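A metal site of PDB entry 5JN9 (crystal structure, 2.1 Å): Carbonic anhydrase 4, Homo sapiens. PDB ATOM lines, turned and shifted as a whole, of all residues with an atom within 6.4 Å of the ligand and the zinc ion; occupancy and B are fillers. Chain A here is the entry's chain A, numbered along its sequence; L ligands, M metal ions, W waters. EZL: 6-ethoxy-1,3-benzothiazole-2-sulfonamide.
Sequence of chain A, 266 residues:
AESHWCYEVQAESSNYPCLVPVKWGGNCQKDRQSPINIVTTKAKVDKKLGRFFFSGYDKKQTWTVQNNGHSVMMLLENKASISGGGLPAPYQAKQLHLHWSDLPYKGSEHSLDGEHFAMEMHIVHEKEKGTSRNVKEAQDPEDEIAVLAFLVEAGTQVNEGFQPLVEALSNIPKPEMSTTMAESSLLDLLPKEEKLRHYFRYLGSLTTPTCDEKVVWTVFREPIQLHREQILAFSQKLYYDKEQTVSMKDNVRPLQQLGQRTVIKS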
ATOM      1  N   TYR A   7       8.737 -37.418  29.004  1.00  0.00           N
ATOM      2  CA  TYR A   7       8.966 -37.144  27.579  1.00  0.00           C
ATOM      3  C   TYR A   7      10.183 -37.956  27.074  1.00  0.00           C
ATOM      4  O   TYR A   7      11.022 -38.454  27.868  1.00  0.00           O
ATOM      5  CB  TYR A   7       9.191 -35.670  27.359  1.00  0.00           C
ATOM      6  CG  TYR A   7       8.007 -34.775  27.668  1.00  0.00           C
ATOM      7  CD1 TYR A   7       6.963 -34.671  26.774  1.00  0.00           C
ATOM      8  CD2 TYR A   7       7.960 -34.014  28.829  1.00  0.00           C
ATOM      9  CE1 TYR A   7       5.899 -33.819  27.016  1.00  0.00           C
ATOM     10  CE2 TYR A   7       6.896 -33.169  29.100  1.00  0.00           C
ATOM     11  CZ  TYR A   7       5.880 -33.069  28.204  1.00  0.00           C
ATOM     12  OH  TYR A   7       4.863 -32.254  28.476  1.00  0.00           O
ATOM     13  N   GLN A  95      -4.241 -21.642  35.225  1.00  0.00           N
ATOM     14  CA  GLN A  95      -2.801 -21.726  35.117  1.00  0.00           C
ATOM     15  C   GLN A  95      -2.326 -21.484  33.707  1.00  0.00           C
ATOM     16  O   GLN A  95      -3.055 -21.753  32.745  1.00  0.00           O
ATOM     17  CB  GLN A  95      -2.288 -23.049  35.656  1.00  0.00           C
ATOM     18  CG  GLN A  95      -2.933 -24.275  35.054  1.00  0.00           C
ATOM     19  CD  GLN A  95      -1.993 -25.048  34.164  1.00  0.00           C
ATOM     20  OE1 GLN A  95      -0.979 -24.505  33.669  1.00  0.00           O
ATOM     21  NE2 GLN A  95      -2.307 -26.338  33.959  1.00  0.00           N
ATOM     22  N   HIS A  97       1.264 -22.225  31.305  1.00  0.00           N
ATOM     23  CA  HIS A  97       2.559 -22.919  31.234  1.00  0.00           C
ATOM     24  C   HIS A  97       3.084 -22.979  29.824  1.00  0.00           C
ATOM     25  O   HIS A  97       2.471 -22.434  28.902  1.00  0.00           O
ATOM     26  CB  HIS A  97       2.463 -24.321  31.863  1.00  0.00           C
ATOM     27  CG  HIS A  97       1.528 -25.214  31.132  1.00  0.00           C
ATOM     28  ND1 HIS A  97       0.198 -25.271  31.436  1.00  0.00           N
ATOM     29  CD2 HIS A  97       1.698 -26.006  30.053  1.00  0.00           C
ATOM     30  CE1 HIS A  97      -0.425 -26.085  30.603  1.00  0.00           C
ATOM     31  NE2 HIS A  97       0.463 -26.543  29.748  1.00  0.00           N
ATOM     32  N   LEU A  98       4.227 -23.630  29.645  1.00  0.00           N
ATOM     33  CA  LEU A  98       4.879 -23.632  28.339  1.00  0.00           C
ATOM     34  C   LEU A  98       5.506 -24.968  27.980  1.00  0.00           C
ATOM     35  O   LEU A  98       5.747 -25.821  28.810  1.00  0.00           O
ATOM     36  CB  LEU A  98       5.941 -22.502  28.250  1.00  0.00           C
ATOM     37  CG  LEU A  98       5.406 -21.062  28.282  1.00  0.00           C
ATOM     38  CD1 LEU A  98       5.452 -20.479  29.672  1.00  0.00           C
ATOM     39  CD2 LEU A  98       6.202 -20.142  27.347  1.00  0.00           C
ATOM     40  N   HIS A  99       5.735 -25.115  26.690  1.00  0.00           N
ATOM     41  CA  HIS A  99       6.445 -26.242  26.115  1.00  0.00           C
ATOM     42  C   HIS A  99       7.466 -25.593  25.192  1.00  0.00           C
ATOM     43  O   HIS A  99       7.148 -24.595  24.549  1.00  0.00           O
ATOM     44  CB  HIS A  99       5.498 -27.083  25.305  1.00  0.00           C
ATOM     45  CG  HIS A  99       4.341 -27.603  26.090  1.00  0.00           C
ATOM     46  ND1 HIS A  99       4.345 -28.859  26.673  1.00  0.00           N
ATOM     47  CD2 HIS A  99       3.143 -27.059  26.398  1.00  0.00           C
ATOM     48  CE1 HIS A  99       3.196 -29.063  27.295  1.00  0.00           C
ATOM     49  NE2 HIS A  99       2.470 -27.986  27.152  1.00  0.00           N
ATOM     50  N   GLU A 109       3.888 -27.650  20.485  1.00  0.00           N
ATOM     51  CA  GLU A 109       3.157 -28.922  20.432  1.00  0.00           C
ATOM     52  C   GLU A 109       2.362 -29.029  19.142  1.00  0.00           C
ATOM     53  O   GLU A 109       2.551 -29.955  18.389  1.00  0.00           O
ATOM     54  CB  GLU A 109       2.276 -29.121  21.669  1.00  0.00           C
ATOM     55  CG  GLU A 109       3.094 -29.165  22.959  1.00  0.00           C
ATOM     56  CD  GLU A 109       2.447 -29.997  24.039  1.00  0.00           C
ATOM     57  OE1 GLU A 109       1.401 -29.541  24.567  1.00  0.00           O
ATOM     58  OE2 GLU A 109       2.995 -31.091  24.338  1.00  0.00           O
ATOM     59  N   GLU A 120       5.417 -23.183  22.651  1.00  0.00           N
ATOM     60  CA  GLU A 120       3.945 -23.043  22.703  1.00  0.00           C
ATOM     61  C   GLU A 120       3.564 -22.759  24.138  1.00  0.00           C
ATOM     62  O   GLU A 120       3.985 -23.470  25.063  1.00  0.00           O
ATOM     63  CB  GLU A 120       3.246 -24.315  22.245  1.00  0.00           C
ATOM     64  CG  GLU A 120       1.754 -24.126  21.989  1.00  0.00           C
ATOM     65  CD  GLU A 120       1.137 -25.242  21.177  1.00  0.00           C
ATOM     66  OE1 GLU A 120       1.847 -25.809  20.298  1.00  0.00           O
ATOM     67  OE2 GLU A 120      -0.065 -25.559  21.418  1.00  0.00           O
ATOM     68  N   MET A 121       2.785 -21.705  24.333  1.00  0.00           N
ATOM     69  CA  MET A 121       2.306 -21.299  25.669  1.00  0.00           C
ATOM     70  C   MET A 121       0.835 -21.643  25.765  1.00  0.00           C
ATOM     71  O   MET A 121       0.058 -21.289  24.869  1.00  0.00           O
ATOM     72  CB  MET A 121       2.476 -19.778  25.857  1.00  0.00           C
ATOM     73  CG  MET A 121       1.875 -19.178  27.136  1.00  0.00           C
ATOM     74  SD  MET A 121       2.469 -17.467  27.332  1.00  0.00           S
ATOM     75  CE  MET A 121       1.127 -16.733  26.473  1.00  0.00           C
ATOM     76  N   HIS A 122       0.459 -22.258  26.885  1.00  0.00           N
ATOM     77  CA  HIS A 122      -0.900 -22.706  27.147  1.00  0.00           C
ATOM     78  C   HIS A 122      -1.481 -22.017  28.356  1.00  0.00           C
ATOM     79  O   HIS A 122      -0.885 -22.085  29.439  1.00  0.00           O
ATOM     80  CB  HIS A 122      -0.904 -24.190  27.368  1.00  0.00           C
ATOM     81  CG  HIS A 122      -0.659 -24.980  26.131  1.00  0.00           C
ATOM     82  ND1 HIS A 122      -0.151 -26.263  26.163  1.00  0.00           N
ATOM     83  CD2 HIS A 122      -0.766 -24.654  24.824  1.00  0.00           C
ATOM     84  CE1 HIS A 122       0.002 -26.709  24.929  1.00  0.00           C
ATOM     85  NE2 HIS A 122      -0.360 -25.744  24.102  1.00  0.00           N
ATOM     86  N   ILE A 123      -2.657 -21.394  28.187  1.00  0.00           N
ATOM     87  CA  ILE A 123      -3.397 -20.790  29.305  1.00  0.00           C
ATOM     88  C   ILE A 123      -4.648 -21.652  29.483  1.00  0.00           C
ATOM     89  O   ILE A 123      -5.465 -21.777  28.551  1.00  0.00           O
ATOM     90  CB  ILE A 123      -3.747 -19.291  29.099  1.00  0.00           C
ATOM     91  CG1 ILE A 123      -2.532 -18.471  28.652  1.00  0.00           C
ATOM     92  CG2 ILE A 123      -4.230 -18.672  30.411  1.00  0.00           C
ATOM     93  CD1 ILE A 123      -2.793 -16.965  28.487  1.00  0.00           C
ATOM     94  N   VAL A 124      -4.762 -22.262  30.669  1.00  0.00           N
ATOM     95  CA  VAL A 124      -5.711 -23.311  30.921  1.00  0.00           C
ATOM     96  C   VAL A 124      -6.849 -22.683  31.685  1.00  0.00           C
ATOM     97  O   VAL A 124      -6.636 -22.077  32.734  1.00  0.00           O
ATOM     98  CB  VAL A 124      -5.082 -24.437  31.769  1.00  0.00           C
ATOM     99  CG1 VAL A 124      -6.080 -25.562  32.055  1.00  0.00           C
ATOM    100  CG2 VAL A 124      -3.820 -24.986  31.116  1.00  0.00           C
ATOM    101  N   ILE A 145     -12.648 -27.774  29.696  1.00  0.00           N
ATOM    102  CA  ILE A 145     -11.410 -27.033  29.755  1.00  0.00           C
ATOM    103  C   ILE A 145     -11.235 -26.369  28.417  1.00  0.00           C
ATOM    104  O   ILE A 145     -11.437 -27.010  27.379  1.00  0.00           O
ATOM    105  CB  ILE A 145     -10.252 -27.981  30.045  1.00  0.00           C
ATOM    106  CG1 ILE A 145     -10.491 -28.646  31.395  1.00  0.00           C
ATOM    107  CG2 ILE A 145      -8.913 -27.238  30.019  1.00  0.00           C
ATOM    108  CD1 ILE A 145      -9.547 -29.764  31.686  1.00  0.00           C
ATOM    109  N   VAL A 147      -8.176 -24.390  26.559  1.00  0.00           N
ATOM    110  CA  VAL A 147      -6.793 -23.998  26.551  1.00  0.00           C
ATOM    111  C   VAL A 147      -6.605 -23.083  25.372  1.00  0.00           C
ATOM    112  O   VAL A 147      -6.990 -23.426  24.255  1.00  0.00           O
ATOM    113  CB  VAL A 147      -5.799 -25.181  26.397  1.00  0.00           C
ATOM    114  CG1 VAL A 147      -4.357 -24.662  26.297  1.00  0.00           C
ATOM    115  CG2 VAL A 147      -5.951 -26.182  27.520  1.00  0.00           C
ATOM    116  N   SER A 205      -7.751 -33.131  23.530  1.00  0.00           N
ATOM    117  CA  SER A 205      -7.314 -33.612  24.827  1.00  0.00           C
ATOM    118  C   SER A 205      -6.289 -32.707  25.497  1.00  0.00           C
ATOM    119  O   SER A 205      -5.740 -31.773  24.914  1.00  0.00           O
ATOM    120  CB  SER A 205      -6.716 -35.012  24.700  1.00  0.00           C
ATOM    121  OG  SER A 205      -5.377 -34.985  24.253  1.00  0.00           O
ATOM    122  N   LEU A 206      -6.021 -33.036  26.758  1.00  0.00           N
ATOM    123  CA  LEU A 206      -4.890 -32.507  27.478  1.00  0.00           C
ATOM    124  C   LEU A 206      -3.646 -33.226  26.863  1.00  0.00           C
ATOM    125  O   LEU A 206      -3.764 -34.348  26.397  1.00  0.00           O
ATOM    126  CB  LEU A 206      -5.067 -32.798  28.969  1.00  0.00           C
ATOM    127  CG  LEU A 206      -6.278 -32.165  29.695  1.00  0.00           C
ATOM    128  CD1 LEU A 206      -6.497 -32.792  31.056  1.00  0.00           C
ATOM    129  CD2 LEU A 206      -6.098 -30.660  29.827  1.00  0.00           C
ATOM    130  N   THR A 207      -2.517 -32.528  26.779  1.00  0.00           N
ATOM    131  CA  THR A 207      -1.300 -33.055  26.154  1.00  0.00           C
ATOM    132  C   THR A 207      -0.319 -33.749  27.108  1.00  0.00           C
ATOM    133  O   THR A 207       0.702 -34.322  26.643  1.00  0.00           O
ATOM    134  CB  THR A 207      -0.539 -31.965  25.348  1.00  0.00           C
ATOM    135  OG1 THR A 207      -0.064 -30.924  26.206  1.00  0.00           O
ATOM    136  CG2 THR A 207      -1.443 -31.377  24.249  1.00  0.00           C
ATOM    137  N   THR A 208      -0.594 -33.694  28.406  1.00  0.00           N
ATOM    138  CA  THR A 208       0.120 -34.541  29.379  1.00  0.00           C
ATOM    139  C   THR A 208      -0.868 -35.456  30.093  1.00  0.00           C
ATOM    140  O   THR A 208      -2.067 -35.164  30.095  1.00  0.00           O
ATOM    141  CB  THR A 208       0.948 -33.715  30.364  1.00  0.00           C
ATOM    142  OG1 THR A 208       0.095 -32.856  31.109  1.00  0.00           O
ATOM    143  CG2 THR A 208       1.982 -32.869  29.609  1.00  0.00           C
ATOM    144  N   PRO A 209      -0.400 -36.587  30.655  1.00  0.00           N
ATOM    145  CA  PRO A 209      -1.360 -37.520  31.281  1.00  0.00           C
ATOM    146  C   PRO A 209      -2.119 -36.894  32.406  1.00  0.00           C
ATOM    147  O   PRO A 209      -1.518 -36.088  33.113  1.00  0.00           O
ATOM    148  CB  PRO A 209      -0.490 -38.658  31.797  1.00  0.00           C
ATOM    149  CG  PRO A 209       0.735 -38.629  30.908  1.00  0.00           C
ATOM    150  CD  PRO A 209       0.973 -37.149  30.658  1.00  0.00           C
ATOM    151  N   THR A 210      -3.391 -37.240  32.599  1.00  0.00           N
ATOM    152  CA  THR A 210      -4.097 -38.361  31.965  1.00  0.00           C
ATOM    153  C   THR A 210      -4.792 -38.072  30.582  1.00  0.00           C
ATOM    154  O   THR A 210      -5.641 -38.827  30.145  1.00  0.00           O
ATOM    155  CB  THR A 210      -5.167 -38.927  32.964  1.00  0.00           C
ATOM    156  OG1 THR A 210      -6.086 -37.903  33.372  1.00  0.00           O
ATOM    157  CG2 THR A 210      -4.532 -39.483  34.162  1.00  0.00           C
ATOM    158  N   CYS A 211      -4.418 -36.998  29.898  1.00  0.00           N
ATOM    159  CA  CYS A 211      -4.816 -36.780  28.486  1.00  0.00           C
ATOM    160  C   CYS A 211      -6.326 -36.808  28.245  1.00  0.00           C
ATOM    161  O   CYS A 211      -6.822 -37.369  27.258  1.00  0.00           O
ATOM    162  CB  CYS A 211      -4.143 -37.795  27.560  1.00  0.00           C
ATOM    163  SG  CYS A 211      -2.322 -37.924  27.698  1.00  0.00           S
ATOM    164  N   VAL A 215     -11.070 -30.974  26.213  1.00  0.00           N
ATOM    165  CA  VAL A 215     -10.514 -29.678  25.935  1.00  0.00           C
ATOM    166  C   VAL A 215     -11.081 -29.097  24.659  1.00  0.00           C
ATOM    167  O   VAL A 215     -11.083 -29.732  23.606  1.00  0.00           O
ATOM    168  CB  VAL A 215      -8.982 -29.751  25.818  1.00  0.00           C
ATOM    169  CG1 VAL A 215      -8.408 -28.374  25.447  1.00  0.00           C
ATOM    170  CG2 VAL A 215      -8.392 -30.271  27.131  1.00  0.00           C
ATOM    171  N   TRP A 217      -9.879 -26.482  22.220  1.00  0.00           N
ATOM    172  CA  TRP A 217      -8.613 -25.864  21.841  1.00  0.00           C
ATOM    173  C   TRP A 217      -8.812 -24.610  21.005  1.00  0.00           C
ATOM    174  O   TRP A 217      -9.652 -24.587  20.083  1.00  0.00           O
ATOM    175  CB  TRP A 217      -7.741 -26.837  21.044  1.00  0.00           C
ATOM    176  CG  TRP A 217      -7.018 -27.740  21.919  1.00  0.00           C
ATOM    177  CD1 TRP A 217      -7.370 -29.013  22.227  1.00  0.00           C
ATOM    178  CD2 TRP A 217      -5.842 -27.449  22.677  1.00  0.00           C
ATOM    179  NE1 TRP A 217      -6.478 -29.539  23.126  1.00  0.00           N
ATOM    180  CE2 TRP A 217      -5.516 -28.596  23.404  1.00  0.00           C
ATOM    181  CE3 TRP A 217      -5.004 -26.316  22.782  1.00  0.00           C
ATOM    182  CZ2 TRP A 217      -4.414 -28.669  24.263  1.00  0.00           C
ATOM    183  CZ3 TRP A 217      -3.892 -26.391  23.588  1.00  0.00           C
ATOM    184  CH2 TRP A 217      -3.597 -27.565  24.319  1.00  0.00           C
HETATM  185  N1  EZL L   1      -0.692 -29.272  28.071  1.00  0.00           N
HETATM  186  C2  EZL L   1      -2.723 -31.219  31.347  1.00  0.00           C
HETATM  187  C3  EZL L   1      -3.180 -30.027  32.076  1.00  0.00           C
HETATM  188  C4  EZL L   1      -3.610 -30.138  33.386  1.00  0.00           C
HETATM  189  C5  EZL L   1      -3.573 -31.383  34.022  1.00  0.00           C
HETATM  190  C8  EZL L   1      -3.891 -30.576  36.344  1.00  0.00           C
HETATM  191  O1  EZL L   1      -2.495 -27.449  28.411  1.00  0.00           O
HETATM  192  O2  EZL L   1      -2.962 -29.496  27.384  1.00  0.00           O
HETATM  193  S1  EZL L   1      -2.190 -28.859  28.414  1.00  0.00           S
HETATM  194  C1  EZL L   1      -2.550 -29.527  29.892  1.00  0.00           C
HETATM  195  N2  EZL L   1      -2.363 -30.841  30.101  1.00  0.00           N
HETATM  196  S2  EZL L   1      -3.199 -28.586  31.223  1.00  0.00           S
HETATM  197  C6  EZL L   1      -3.127 -32.522  33.349  1.00  0.00           C
HETATM  198  C7  EZL L   1      -2.715 -32.436  32.033  1.00  0.00           C
HETATM  199  O3  EZL L   1      -3.978 -31.576  35.319  1.00  0.00           O
HETATM  200  C9  EZL L   1      -3.243 -31.173  37.582  1.00  0.00           C
HETATM  201 ZN    ZN M   1       0.479 -27.554  27.795  1.00  0.00          ZN
HETATM  202  O   HOH W   1       0.447 -30.154  30.980  1.00  0.00           O
HETATM  203  O   HOH W   2      -0.105 -28.718  33.115  1.00  0.00           O
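N1 of the ligand is bound to the zinc ion. The zinc ion is bound by NE2 of His 99 (2.1 Å). The zinc ion is bound by ND1 of His 122 (2.2 Å). The zinc ion is bound by NE2 of His 97 (2.2 Å).
A ring nitrogen (NE2) of His 99 sits close to the side-chain carboxylate (OE1) of Glu 109 (3.2 Å). The backbone carbonyl oxygen (O) of Glu 120 sits at hydrogen-bond distance from the backbone NH (N) of His 99 (2.9 Å). The side-chain carboxylate of Glu 120 is in hydrogen-bond range of a ring nitrogen (NE2) of His 122, at 2.7 Å. ND1 of His 97 sits at hydrogen-bond distance from OE1 of Gln 95. The side-chain hydroxyl (OG1) of Thr 207 sits at hydrogen-bond distance from the side-chain carboxylate (OE1) of Glu 109 (2.6 Å). The backbone carbonyl oxygen of Ser 205 sits at hydrogen-bond distance from the indole nitrogen of Trp 217 (3.0 Å). O of Gln 95 sits at hydrogen-bond distance from N of Val 124 (2.7 Å). N of Glu 109 lies within hydrogen-bond range of OE1 of Glu 120, at 2.8 Å.
Residues that only touch the zinc ion: Thr 207 and Glu 109. Along chain A the residues within 4 Å of the zinc ion span positions 97 to 207. The nearest printed residue that does not touch the zinc ion is Trp 217 (5.4 Å).
Val 124 touches the ligand. Val 147 touches the ligand (CG2 to O1, 3.8 Å). Leu 206 touches the ligand. Pro 209 touches the ligand (O to C6, 3.9 Å). Trp 217 touches the ligand (CZ2 to O2, 3.5 Å). Hydrophobic or aromatic side chains that line the ligand: His 97, His 99, His 122, Val 124, Val 147, Leu 206 and Trp 217. The nearest printed residue that does not touch the ligand is Glu 109 (4.1 Å).
The backbone NH (N) of Thr 207 lies within hydrogen-bond range of an oxygen (O2) of the ligand (3.1 Å). The side-chain hydroxyl (OG1) of Thr 207 sits at hydrogen-bond distance from an oxygen (O2) of the ligand, at 3.4 Å. A nitrogen (N2) of the ligand sits close to the side-chain hydroxyl of Thr 208, at 3.3 Å. A sulfur (S2) of the ligand lies close to the side-chain amide nitrogen (NE2) of Gln 95, at 3.7 Å.
Water W1 bridges the side-chain hydroxyl (OG1) of Thr 208 (2.7 Å) and a nitrogen (N2) of the ligand (3.0 Å). Water W2 lies within hydrogen-bond range of NE2 of Gln 95 (3.4 Å) and S2 of the ligand (3.6 Å).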
